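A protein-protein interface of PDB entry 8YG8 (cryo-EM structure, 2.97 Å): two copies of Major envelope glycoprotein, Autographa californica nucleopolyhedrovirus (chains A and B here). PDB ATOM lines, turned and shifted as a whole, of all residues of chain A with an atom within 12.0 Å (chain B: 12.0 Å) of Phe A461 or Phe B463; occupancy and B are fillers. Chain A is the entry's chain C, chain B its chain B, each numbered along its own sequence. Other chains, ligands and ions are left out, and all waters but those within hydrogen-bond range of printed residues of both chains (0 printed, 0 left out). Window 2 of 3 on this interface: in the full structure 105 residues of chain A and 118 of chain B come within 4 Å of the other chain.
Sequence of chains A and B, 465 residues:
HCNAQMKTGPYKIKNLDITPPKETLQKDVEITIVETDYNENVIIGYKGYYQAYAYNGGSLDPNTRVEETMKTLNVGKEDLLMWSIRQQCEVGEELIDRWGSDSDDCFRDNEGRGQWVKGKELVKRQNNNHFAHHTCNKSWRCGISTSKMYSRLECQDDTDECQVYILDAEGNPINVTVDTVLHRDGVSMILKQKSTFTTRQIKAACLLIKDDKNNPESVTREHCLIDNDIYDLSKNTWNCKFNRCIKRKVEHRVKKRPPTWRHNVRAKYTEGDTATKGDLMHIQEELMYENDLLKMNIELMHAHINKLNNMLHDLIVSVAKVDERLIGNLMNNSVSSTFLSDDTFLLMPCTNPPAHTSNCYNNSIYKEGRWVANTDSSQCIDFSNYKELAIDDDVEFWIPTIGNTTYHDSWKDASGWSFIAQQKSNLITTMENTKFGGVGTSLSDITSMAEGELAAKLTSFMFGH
Among the printed residues, pairs that only touch across the chains: Leu A454 with Glu B453 (3.5 Å), Lys A457 with Ala B456 (3.7 Å), Leu A458 with Glu B453 (3.8 Å), Phe A461 with Ser B460 (3.0 Å) and Phe A461 with Phe B463 (3.4 Å).
NE2 of His B465 sits at hydrogen-bond distance from OG of Ser B460.
Leu A454 touches Glu B453, but with the chains exchanged Glu A453 does not touch Leu B454 (11.0 Å).
Lys B457 touches its own counterpart, Lys A457.
Leu A458 touches Glu B453, but with the chains exchanged Glu A453 does not touch Leu B458 (12.3 Å).
Phe A461 touches Phe B463, but with the chains exchanged Phe A463 does not touch Phe B461 (13.2 Å).
14 positions are printed for both chains.
Of the 7 pairs that touch across the chains among the printed residues, 1 has its exchanged pair printed and touching as well.
Of the printed residues of chain B, Leu A454 touches Glu B453 (3.5 Å).
Ala A455 touches none of the printed residues of chain B.
Printed residues of chain B within 4 Å of Lys A457: Glu B453, Ala B456 and Lys B457.
No residue of chain B comes within 4 Å of Thr A459.
Ser A460 touches none of the printed residues of chain B.
Of the printed residues of chain B, Phe A461 touches Ser B460 and Phe B463.
Met A462 touches none of the printed residues of chain B.
No residue of chain B comes within 4 Å of Phe A463.
No residue of chain B comes within 4 Å of Gly A464.
Printed residues of chain A within 4 Å of Glu B453: Leu A454 (3.5 Å), Lys A457 (2.5 Å) and Leu A458 (3.8 Å).
Printed residues of chain A within 4 Å of Lys B457: Lys A457.
Thr B459 touches none of the printed residues of chain A.
Ser B460 touches just one residue of chain A: Phe A461 (3.0 Å).
No residue of chain A comes within 4 Å of Met B462.
Phe B463 touches just one residue of chain A: Phe A461 (3.4 Å).
No residue of chain A comes within 4 Å of Gly B464.
His B465 touches none of the printed residues of chain A.
The nearest printed residue of chain B that does not touch Leu A454 is Leu B454 (6.5 Å).
OE2 of Glu B453 is in salt-bridge range of NZ of Lys A457, at 2.5 Å.
The backbone NH of Lys B457 lies close to the side-chain amino group of Lys A457 (3.4 Å).
Printed residues of chain A that touch a printed residue of chain B: Leu A454, Lys A457, Leu A458 and Phe A461.
Along chain B the printed residues that touch a printed residue of chain A span positions 453 to 463.
Among the printed residues, Asp or Glu carboxylates within 4 Å of a Lys or Arg side-chain nitrogen of the other chain: Lys A457 with Glu B453.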
ATOM      1  N   GLY A 452      18.805   3.960   7.340  1.00  0.00           N
ATOM      2  CA  GLY A 452      19.457   3.790   8.622  1.00  0.00           C
ATOM      3  C   GLY A 452      19.774   2.350   8.958  1.00  0.00           C
ATOM      4  O   GLY A 452      20.947   1.975   9.061  1.00  0.00           O
ATOM      5  N   GLU A 453      18.733   1.532   9.124  1.00  0.00           N
ATOM      6  CA  GLU A 453      18.945   0.123   9.433  1.00  0.00           C
ATOM      7  C   GLU A 453      19.669  -0.602   8.309  1.00  0.00           C
ATOM      8  O   GLU A 453      20.432  -1.533   8.575  1.00  0.00           O
ATOM      9  CB  GLU A 453      17.613  -0.560   9.739  1.00  0.00           C
ATOM     10  CG  GLU A 453      16.951  -0.082  11.019  1.00  0.00           C
ATOM     11  CD  GLU A 453      16.173   1.198  10.829  1.00  0.00           C
ATOM     12  OE1 GLU A 453      16.103   1.678   9.682  1.00  0.00           O
ATOM     13  OE2 GLU A 453      15.633   1.724  11.823  1.00  0.00           O
ATOM     14  N   LEU A 454      19.452  -0.197   7.057  1.00  0.00           N
ATOM     15  CA  LEU A 454      20.144  -0.845   5.947  1.00  0.00           C
ATOM     16  C   LEU A 454      21.654  -0.667   6.067  1.00  0.00           C
ATOM     17  O   LEU A 454      22.415  -1.644   6.027  1.00  0.00           O
ATOM     18  CB  LEU A 454      19.634  -0.290   4.618  1.00  0.00           C
ATOM     19  CG  LEU A 454      18.438  -1.004   3.982  1.00  0.00           C
ATOM     20  CD1 LEU A 454      18.791  -2.438   3.648  1.00  0.00           C
ATOM     21  CD2 LEU A 454      17.212  -0.953   4.882  1.00  0.00           C
ATOM     22  N   ALA A 455      22.104   0.579   6.239  1.00  0.00           N
ATOM     23  CA  ALA A 455      23.529   0.836   6.408  1.00  0.00           C
ATOM     24  C   ALA A 455      24.051   0.209   7.694  1.00  0.00           C
ATOM     25  O   ALA A 455      25.190  -0.273   7.738  1.00  0.00           O
ATOM     26  CB  ALA A 455      23.798   2.340   6.394  1.00  0.00           C
ATOM     27  N   ALA A 456      23.238   0.212   8.754  1.00  0.00           N
ATOM     28  CA  ALA A 456      23.665  -0.392  10.011  1.00  0.00           C
ATOM     29  C   ALA A 456      23.929  -1.881   9.837  1.00  0.00           C
ATOM     30  O   ALA A 456      24.976  -2.388  10.252  1.00  0.00           O
ATOM     31  CB  ALA A 456      22.614  -0.151  11.094  1.00  0.00           C
ATOM     32  N   LYS A 457      22.995  -2.596   9.205  1.00  0.00           N
ATOM     33  CA  LYS A 457      23.191  -4.016   8.937  1.00  0.00           C
ATOM     34  C   LYS A 457      24.405  -4.240   8.051  1.00  0.00           C
ATOM     35  O   LYS A 457      25.209  -5.148   8.300  1.00  0.00           O
ATOM     36  CB  LYS A 457      21.935  -4.608   8.290  1.00  0.00           C
ATOM     37  CG  LYS A 457      22.139  -5.972   7.632  1.00  0.00           C
ATOM     38  CD  LYS A 457      22.370  -5.847   6.125  1.00  0.00           C
ATOM     39  CE  LYS A 457      22.735  -7.182   5.497  1.00  0.00           C
ATOM     40  NZ  LYS A 457      23.023  -7.063   4.043  1.00  0.00           N
ATOM     41  N   LEU A 458      24.550  -3.423   7.006  1.00  0.00           N
ATOM     42  CA  LEU A 458      25.669  -3.610   6.092  1.00  0.00           C
ATOM     43  C   LEU A 458      26.994  -3.485   6.830  1.00  0.00           C
ATOM     44  O   LEU A 458      27.830  -4.392   6.779  1.00  0.00           O
ATOM     45  CB  LEU A 458      25.575  -2.603   4.942  1.00  0.00           C
ATOM     46  CG  LEU A 458      26.545  -2.724   3.762  1.00  0.00           C
ATOM     47  CD1 LEU A 458      25.908  -2.134   2.516  1.00  0.00           C
ATOM     48  CD2 LEU A 458      27.870  -2.021   4.041  1.00  0.00           C
ATOM     49  N   THR A 459      27.182  -2.383   7.559  1.00  0.00           N
ATOM     50  CA  THR A 459      28.430  -2.184   8.290  1.00  0.00           C
ATOM     51  C   THR A 459      28.635  -3.265   9.341  1.00  0.00           C
ATOM     52  O   THR A 459      29.741  -3.812   9.474  1.00  0.00           O
ATOM     53  CB  THR A 459      28.446  -0.801   8.941  1.00  0.00           C
ATOM     54  OG1 THR A 459      28.351   0.205   7.924  1.00  0.00           O
ATOM     55  CG2 THR A 459      29.725  -0.594   9.739  1.00  0.00           C
ATOM     56  N   SER A 460      27.579  -3.589  10.095  1.00  0.00           N
ATOM     57  CA  SER A 460      27.688  -4.575  11.162  1.00  0.00           C
ATOM     58  C   SER A 460      28.170  -5.908  10.620  1.00  0.00           C
ATOM     59  O   SER A 460      29.123  -6.495  11.143  1.00  0.00           O
ATOM     60  CB  SER A 460      26.341  -4.737  11.866  1.00  0.00           C
ATOM     61  OG  SER A 460      26.395  -5.775  12.830  1.00  0.00           O
ATOM     62  N   PHE A 461      27.547  -6.385   9.544  1.00  0.00           N
ATOM     63  CA  PHE A 461      27.951  -7.673   9.005  1.00  0.00           C
ATOM     64  C   PHE A 461      29.298  -7.603   8.298  1.00  0.00           C
ATOM     65  O   PHE A 461      30.015  -8.610   8.255  1.00  0.00           O
ATOM     66  CB  PHE A 461      26.874  -8.218   8.067  1.00  0.00           C
ATOM     67  CG  PHE A 461      27.002  -9.683   7.812  1.00  0.00           C
ATOM     68  CD1 PHE A 461      26.752 -10.595   8.824  1.00  0.00           C
ATOM     69  CD2 PHE A 461      27.370 -10.158   6.566  1.00  0.00           C
ATOM     70  CE1 PHE A 461      26.871 -11.949   8.602  1.00  0.00           C
ATOM     71  CE2 PHE A 461      27.487 -11.511   6.335  1.00  0.00           C
ATOM     72  CZ  PHE A 461      27.237 -12.408   7.356  1.00  0.00           C
ATOM     73  N   MET A 462      29.679  -6.440   7.757  1.00  0.00           N
ATOM     74  CA  MET A 462      31.003  -6.338   7.151  1.00  0.00           C
ATOM     75  C   MET A 462      32.115  -6.459   8.187  1.00  0.00           C
ATOM     76  O   MET A 462      33.088  -7.189   7.965  1.00  0.00           O
ATOM     77  CB  MET A 462      31.143  -5.041   6.353  1.00  0.00           C
ATOM     78  CG  MET A 462      30.241  -4.955   5.127  1.00  0.00           C
ATOM     79  SD  MET A 462      30.582  -6.245   3.910  1.00  0.00           S
ATOM     80  CE  MET A 462      29.244  -7.399   4.208  1.00  0.00           C
ATOM     81  N   PHE A 463      32.006  -5.768   9.331  1.00  0.00           N
ATOM     82  CA  PHE A 463      33.106  -5.966  10.277  1.00  0.00           C
ATOM     83  C   PHE A 463      32.903  -7.198  11.153  1.00  0.00           C
ATOM     84  O   PHE A 463      33.844  -7.610  11.841  1.00  0.00           O
ATOM     85  CB  PHE A 463      33.403  -4.744  11.172  1.00  0.00           C
ATOM     86  CG  PHE A 463      32.302  -4.346  12.122  1.00  0.00           C
ATOM     87  CD1 PHE A 463      31.331  -3.441  11.751  1.00  0.00           C
ATOM     88  CD2 PHE A 463      32.275  -4.854  13.410  1.00  0.00           C
ATOM     89  CE1 PHE A 463      30.344  -3.058  12.641  1.00  0.00           C
ATOM     90  CE2 PHE A 463      31.282  -4.484  14.298  1.00  0.00           C
ATOM     91  CZ  PHE A 463      30.311  -3.590  13.908  1.00  0.00           C
ATOM     92  N   GLY A 464      31.709  -7.799  11.145  1.00  0.00           N
ATOM     93  CA  GLY A 464      31.553  -9.117  11.734  1.00  0.00           C
ATOM     94  C   GLY A 464      32.058 -10.243  10.861  1.00  0.00           C
ATOM     95  O   GLY A 464      32.311 -11.340  11.367  1.00  0.00           O
ATOM     96  N   HIS A 465      32.198  -9.998   9.562  1.00  0.00           N
ATOM     97  CA  HIS A 465      32.811 -10.960   8.658  1.00  0.00           C
ATOM     98  C   HIS A 465      34.322 -10.972   8.848  1.00  0.00           C
ATOM     99  O   HIS A 465      34.918  -9.946   9.173  1.00  0.00           O
ATOM    100  CB  HIS A 465      32.462 -10.629   7.207  1.00  0.00           C
ATOM    101  CG  HIS A 465      33.200 -11.461   6.206  1.00  0.00           C
ATOM    102  ND1 HIS A 465      33.099 -12.834   6.161  1.00  0.00           N
ATOM    103  CD2 HIS A 465      34.057 -11.114   5.216  1.00  0.00           C
ATOM    104  CE1 HIS A 465      33.860 -13.297   5.185  1.00  0.00           C
ATOM    105  NE2 HIS A 465      34.451 -12.274   4.596  1.00  0.00           N
ATOM    106  N   GLY B 452      20.475  -6.208  -4.963  1.00  0.00           N
ATOM    107  CA  GLY B 452      21.782  -6.606  -4.467  1.00  0.00           C
ATOM    108  C   GLY B 452      21.846  -6.648  -2.952  1.00  0.00           C
ATOM    109  O   GLY B 452      22.419  -7.568  -2.369  1.00  0.00           O
ATOM    110  N   GLU B 453      21.257  -5.648  -2.294  1.00  0.00           N
ATOM    111  CA  GLU B 453      21.269  -5.631  -0.835  1.00  0.00           C
ATOM    112  C   GLU B 453      20.415  -6.749  -0.250  1.00  0.00           C
ATOM    113  O   GLU B 453      20.785  -7.336   0.775  1.00  0.00           O
ATOM    114  CB  GLU B 453      20.799  -4.273  -0.319  1.00  0.00           C
ATOM    115  CG  GLU B 453      20.617  -4.212   1.186  1.00  0.00           C
ATOM    116  CD  GLU B 453      21.857  -4.633   1.954  1.00  0.00           C
ATOM    117  OE1 GLU B 453      22.981  -4.397   1.462  1.00  0.00           O
ATOM    118  OE2 GLU B 453      21.704  -5.208   3.050  1.00  0.00           O
ATOM    119  N   LEU B 454      19.278  -7.059  -0.874  1.00  0.00           N
ATOM    120  CA  LEU B 454      18.476  -8.189  -0.418  1.00  0.00           C
ATOM    121  C   LEU B 454      19.244  -9.496  -0.568  1.00  0.00           C
ATOM    122  O   LEU B 454      19.196 -10.359   0.317  1.00  0.00           O
ATOM    123  CB  LEU B 454      17.156  -8.238  -1.188  1.00  0.00           C
ATOM    124  CG  LEU B 454      16.105  -9.269  -0.765  1.00  0.00           C
ATOM    125  CD1 LEU B 454      14.710  -8.696  -0.947  1.00  0.00           C
ATOM    126  CD2 LEU B 454      16.245 -10.562  -1.557  1.00  0.00           C
ATOM    127  N   ALA B 455      19.958  -9.658  -1.683  1.00  0.00           N
ATOM    128  CA  ALA B 455      20.787 -10.847  -1.860  1.00  0.00           C
ATOM    129  C   ALA B 455      21.909 -10.900  -0.831  1.00  0.00           C
ATOM    130  O   ALA B 455      22.245 -11.983  -0.334  1.00  0.00           O
ATOM    131  CB  ALA B 455      21.359 -10.883  -3.275  1.00  0.00           C
ATOM    132  N   ALA B 456      22.501  -9.749  -0.508  1.00  0.00           N
ATOM    133  CA  ALA B 456      23.533  -9.705   0.522  1.00  0.00           C
ATOM    134  C   ALA B 456      22.972 -10.113   1.877  1.00  0.00           C
ATOM    135  O   ALA B 456      23.624 -10.839   2.632  1.00  0.00           O
ATOM    136  CB  ALA B 456      24.147  -8.307   0.593  1.00  0.00           C
ATOM    137  N   LYS B 457      21.763  -9.653   2.200  1.00  0.00           N
ATOM    138  CA  LYS B 457      21.120 -10.068   3.444  1.00  0.00           C
ATOM    139  C   LYS B 457      20.842 -11.568   3.443  1.00  0.00           C
ATOM    140  O   LYS B 457      21.023 -12.243   4.465  1.00  0.00           O
ATOM    141  CB  LYS B 457      19.828  -9.275   3.652  1.00  0.00           C
ATOM    142  CG  LYS B 457      18.903  -9.813   4.740  1.00  0.00           C
ATOM    143  CD  LYS B 457      19.630 -10.035   6.059  1.00  0.00           C
ATOM    144  CE  LYS B 457      19.919  -8.735   6.765  1.00  0.00           C
ATOM    145  NZ  LYS B 457      20.698  -8.968   8.009  1.00  0.00           N
ATOM    146  N   LEU B 458      20.388 -12.107   2.310  1.00  0.00           N
ATOM    147  CA  LEU B 458      20.134 -13.543   2.229  1.00  0.00           C
ATOM    148  C   LEU B 458      21.412 -14.342   2.449  1.00  0.00           C
ATOM    149  O   LEU B 458      21.414 -15.340   3.181  1.00  0.00           O
ATOM    150  CB  LEU B 458      19.511 -13.892   0.879  1.00  0.00           C
ATOM    151  CG  LEU B 458      19.308 -15.385   0.611  1.00  0.00           C
ATOM    152  CD1 LEU B 458      18.336 -15.988   1.615  1.00  0.00           C
ATOM    153  CD2 LEU B 458      18.829 -15.620  -0.814  1.00  0.00           C
ATOM    154  N   THR B 459      22.511 -13.919   1.823  1.00  0.00           N
ATOM    155  CA  THR B 459      23.791 -14.588   2.033  1.00  0.00           C
ATOM    156  C   THR B 459      24.240 -14.457   3.484  1.00  0.00           C
ATOM    157  O   THR B 459      24.765 -15.410   4.073  1.00  0.00           O
ATOM    158  CB  THR B 459      24.846 -14.017   1.084  1.00  0.00           C
ATOM    159  OG1 THR B 459      24.294 -13.903  -0.233  1.00  0.00           O
ATOM    160  CG2 THR B 459      26.067 -14.924   1.037  1.00  0.00           C
ATOM    161  N   SER B 460      24.052 -13.270   4.066  1.00  0.00           N
ATOM    162  CA  SER B 460      24.349 -13.055   5.477  1.00  0.00           C
ATOM    163  C   SER B 460      23.633 -14.080   6.339  1.00  0.00           C
ATOM    164  O   SER B 460      24.253 -14.767   7.159  1.00  0.00           O
ATOM    165  CB  SER B 460      23.942 -11.636   5.876  1.00  0.00           C
ATOM    166  OG  SER B 460      24.249 -11.369   7.231  1.00  0.00           O
ATOM    167  N   PHE B 461      22.321 -14.210   6.143  1.00  0.00           N
ATOM    168  CA  PHE B 461      21.556 -15.218   6.866  1.00  0.00           C
ATOM    169  C   PHE B 461      22.147 -16.605   6.656  1.00  0.00           C
ATOM    170  O   PHE B 461      22.469 -17.304   7.624  1.00  0.00           O
ATOM    171  CB  PHE B 461      20.093 -15.189   6.423  1.00  0.00           C
ATOM    172  CG  PHE B 461      19.182 -16.013   7.288  1.00  0.00           C
ATOM    173  CD1 PHE B 461      18.945 -15.659   8.606  1.00  0.00           C
ATOM    174  CD2 PHE B 461      18.570 -17.149   6.785  1.00  0.00           C
ATOM    175  CE1 PHE B 461      18.110 -16.419   9.404  1.00  0.00           C
ATOM    176  CE2 PHE B 461      17.734 -17.914   7.578  1.00  0.00           C
ATOM    177  CZ  PHE B 461      17.505 -17.548   8.888  1.00  0.00           C
ATOM    178  N   MET B 462      22.351 -16.993   5.395  1.00  0.00           N
ATOM    179  CA  MET B 462      22.747 -18.368   5.106  1.00  0.00           C
ATOM    180  C   MET B 462      24.084 -18.736   5.741  1.00  0.00           C
ATOM    181  O   MET B 462      24.194 -19.810   6.344  1.00  0.00           O
ATOM    182  CB  MET B 462      22.807 -18.616   3.598  1.00  0.00           C
ATOM    183  CG  MET B 462      21.464 -18.551   2.890  1.00  0.00           C
ATOM    184  SD  MET B 462      21.594 -18.925   1.128  1.00  0.00           S
ATOM    185  CE  MET B 462      22.348 -17.434   0.493  1.00  0.00           C
ATOM    186  N   PHE B 463      25.103 -17.883   5.634  1.00  0.00           N
ATOM    187  CA  PHE B 463      26.435 -18.293   6.069  1.00  0.00           C
ATOM    188  C   PHE B 463      26.845 -17.707   7.419  1.00  0.00           C
ATOM    189  O   PHE B 463      27.935 -18.022   7.906  1.00  0.00           O
ATOM    190  CB  PHE B 463      27.483 -17.990   4.981  1.00  0.00           C
ATOM    191  CG  PHE B 463      28.110 -16.615   5.052  1.00  0.00           C
ATOM    192  CD1 PHE B 463      29.219 -16.375   5.851  1.00  0.00           C
ATOM    193  CD2 PHE B 463      27.635 -15.583   4.265  1.00  0.00           C
ATOM    194  CE1 PHE B 463      29.802 -15.125   5.900  1.00  0.00           C
ATOM    195  CE2 PHE B 463      28.214 -14.330   4.309  1.00  0.00           C
ATOM    196  CZ  PHE B 463      29.301 -14.104   5.125  1.00  0.00           C
ATOM    197  N   GLY B 464      25.996 -16.909   8.066  1.00  0.00           N
ATOM    198  CA  GLY B 464      26.350 -16.436   9.387  1.00  0.00           C
ATOM    199  C   GLY B 464      25.305 -16.713  10.446  1.00  0.00           C
ATOM    200  O   GLY B 464      25.609 -16.684  11.641  1.00  0.00           O
ATOM    201  N   HIS B 465      24.071 -16.979  10.029  1.00  0.00           N
ATOM    202  CA  HIS B 465      22.970 -17.111  10.970  1.00  0.00           C
ATOM    203  C   HIS B 465      22.498 -18.560  11.047  1.00  0.00           C
ATOM    204  O   HIS B 465      21.919 -18.983  12.048  1.00  0.00           O
ATOM    205  CB  HIS B 465      21.807 -16.196  10.570  1.00  0.00           C
ATOM    206  CG  HIS B 465      22.211 -14.784  10.269  1.00  0.00           C
ATOM    207  ND1 HIS B 465      21.321 -13.846   9.793  1.00  0.00           N
ATOM    208  CD2 HIS B 465      23.400 -14.147  10.385  1.00  0.00           C
ATOM    209  CE1 HIS B 465      21.946 -12.696   9.617  1.00  0.00           C
ATOM    210  NE2 HIS B 465      23.210 -12.851   9.971  1.00  0.00           N
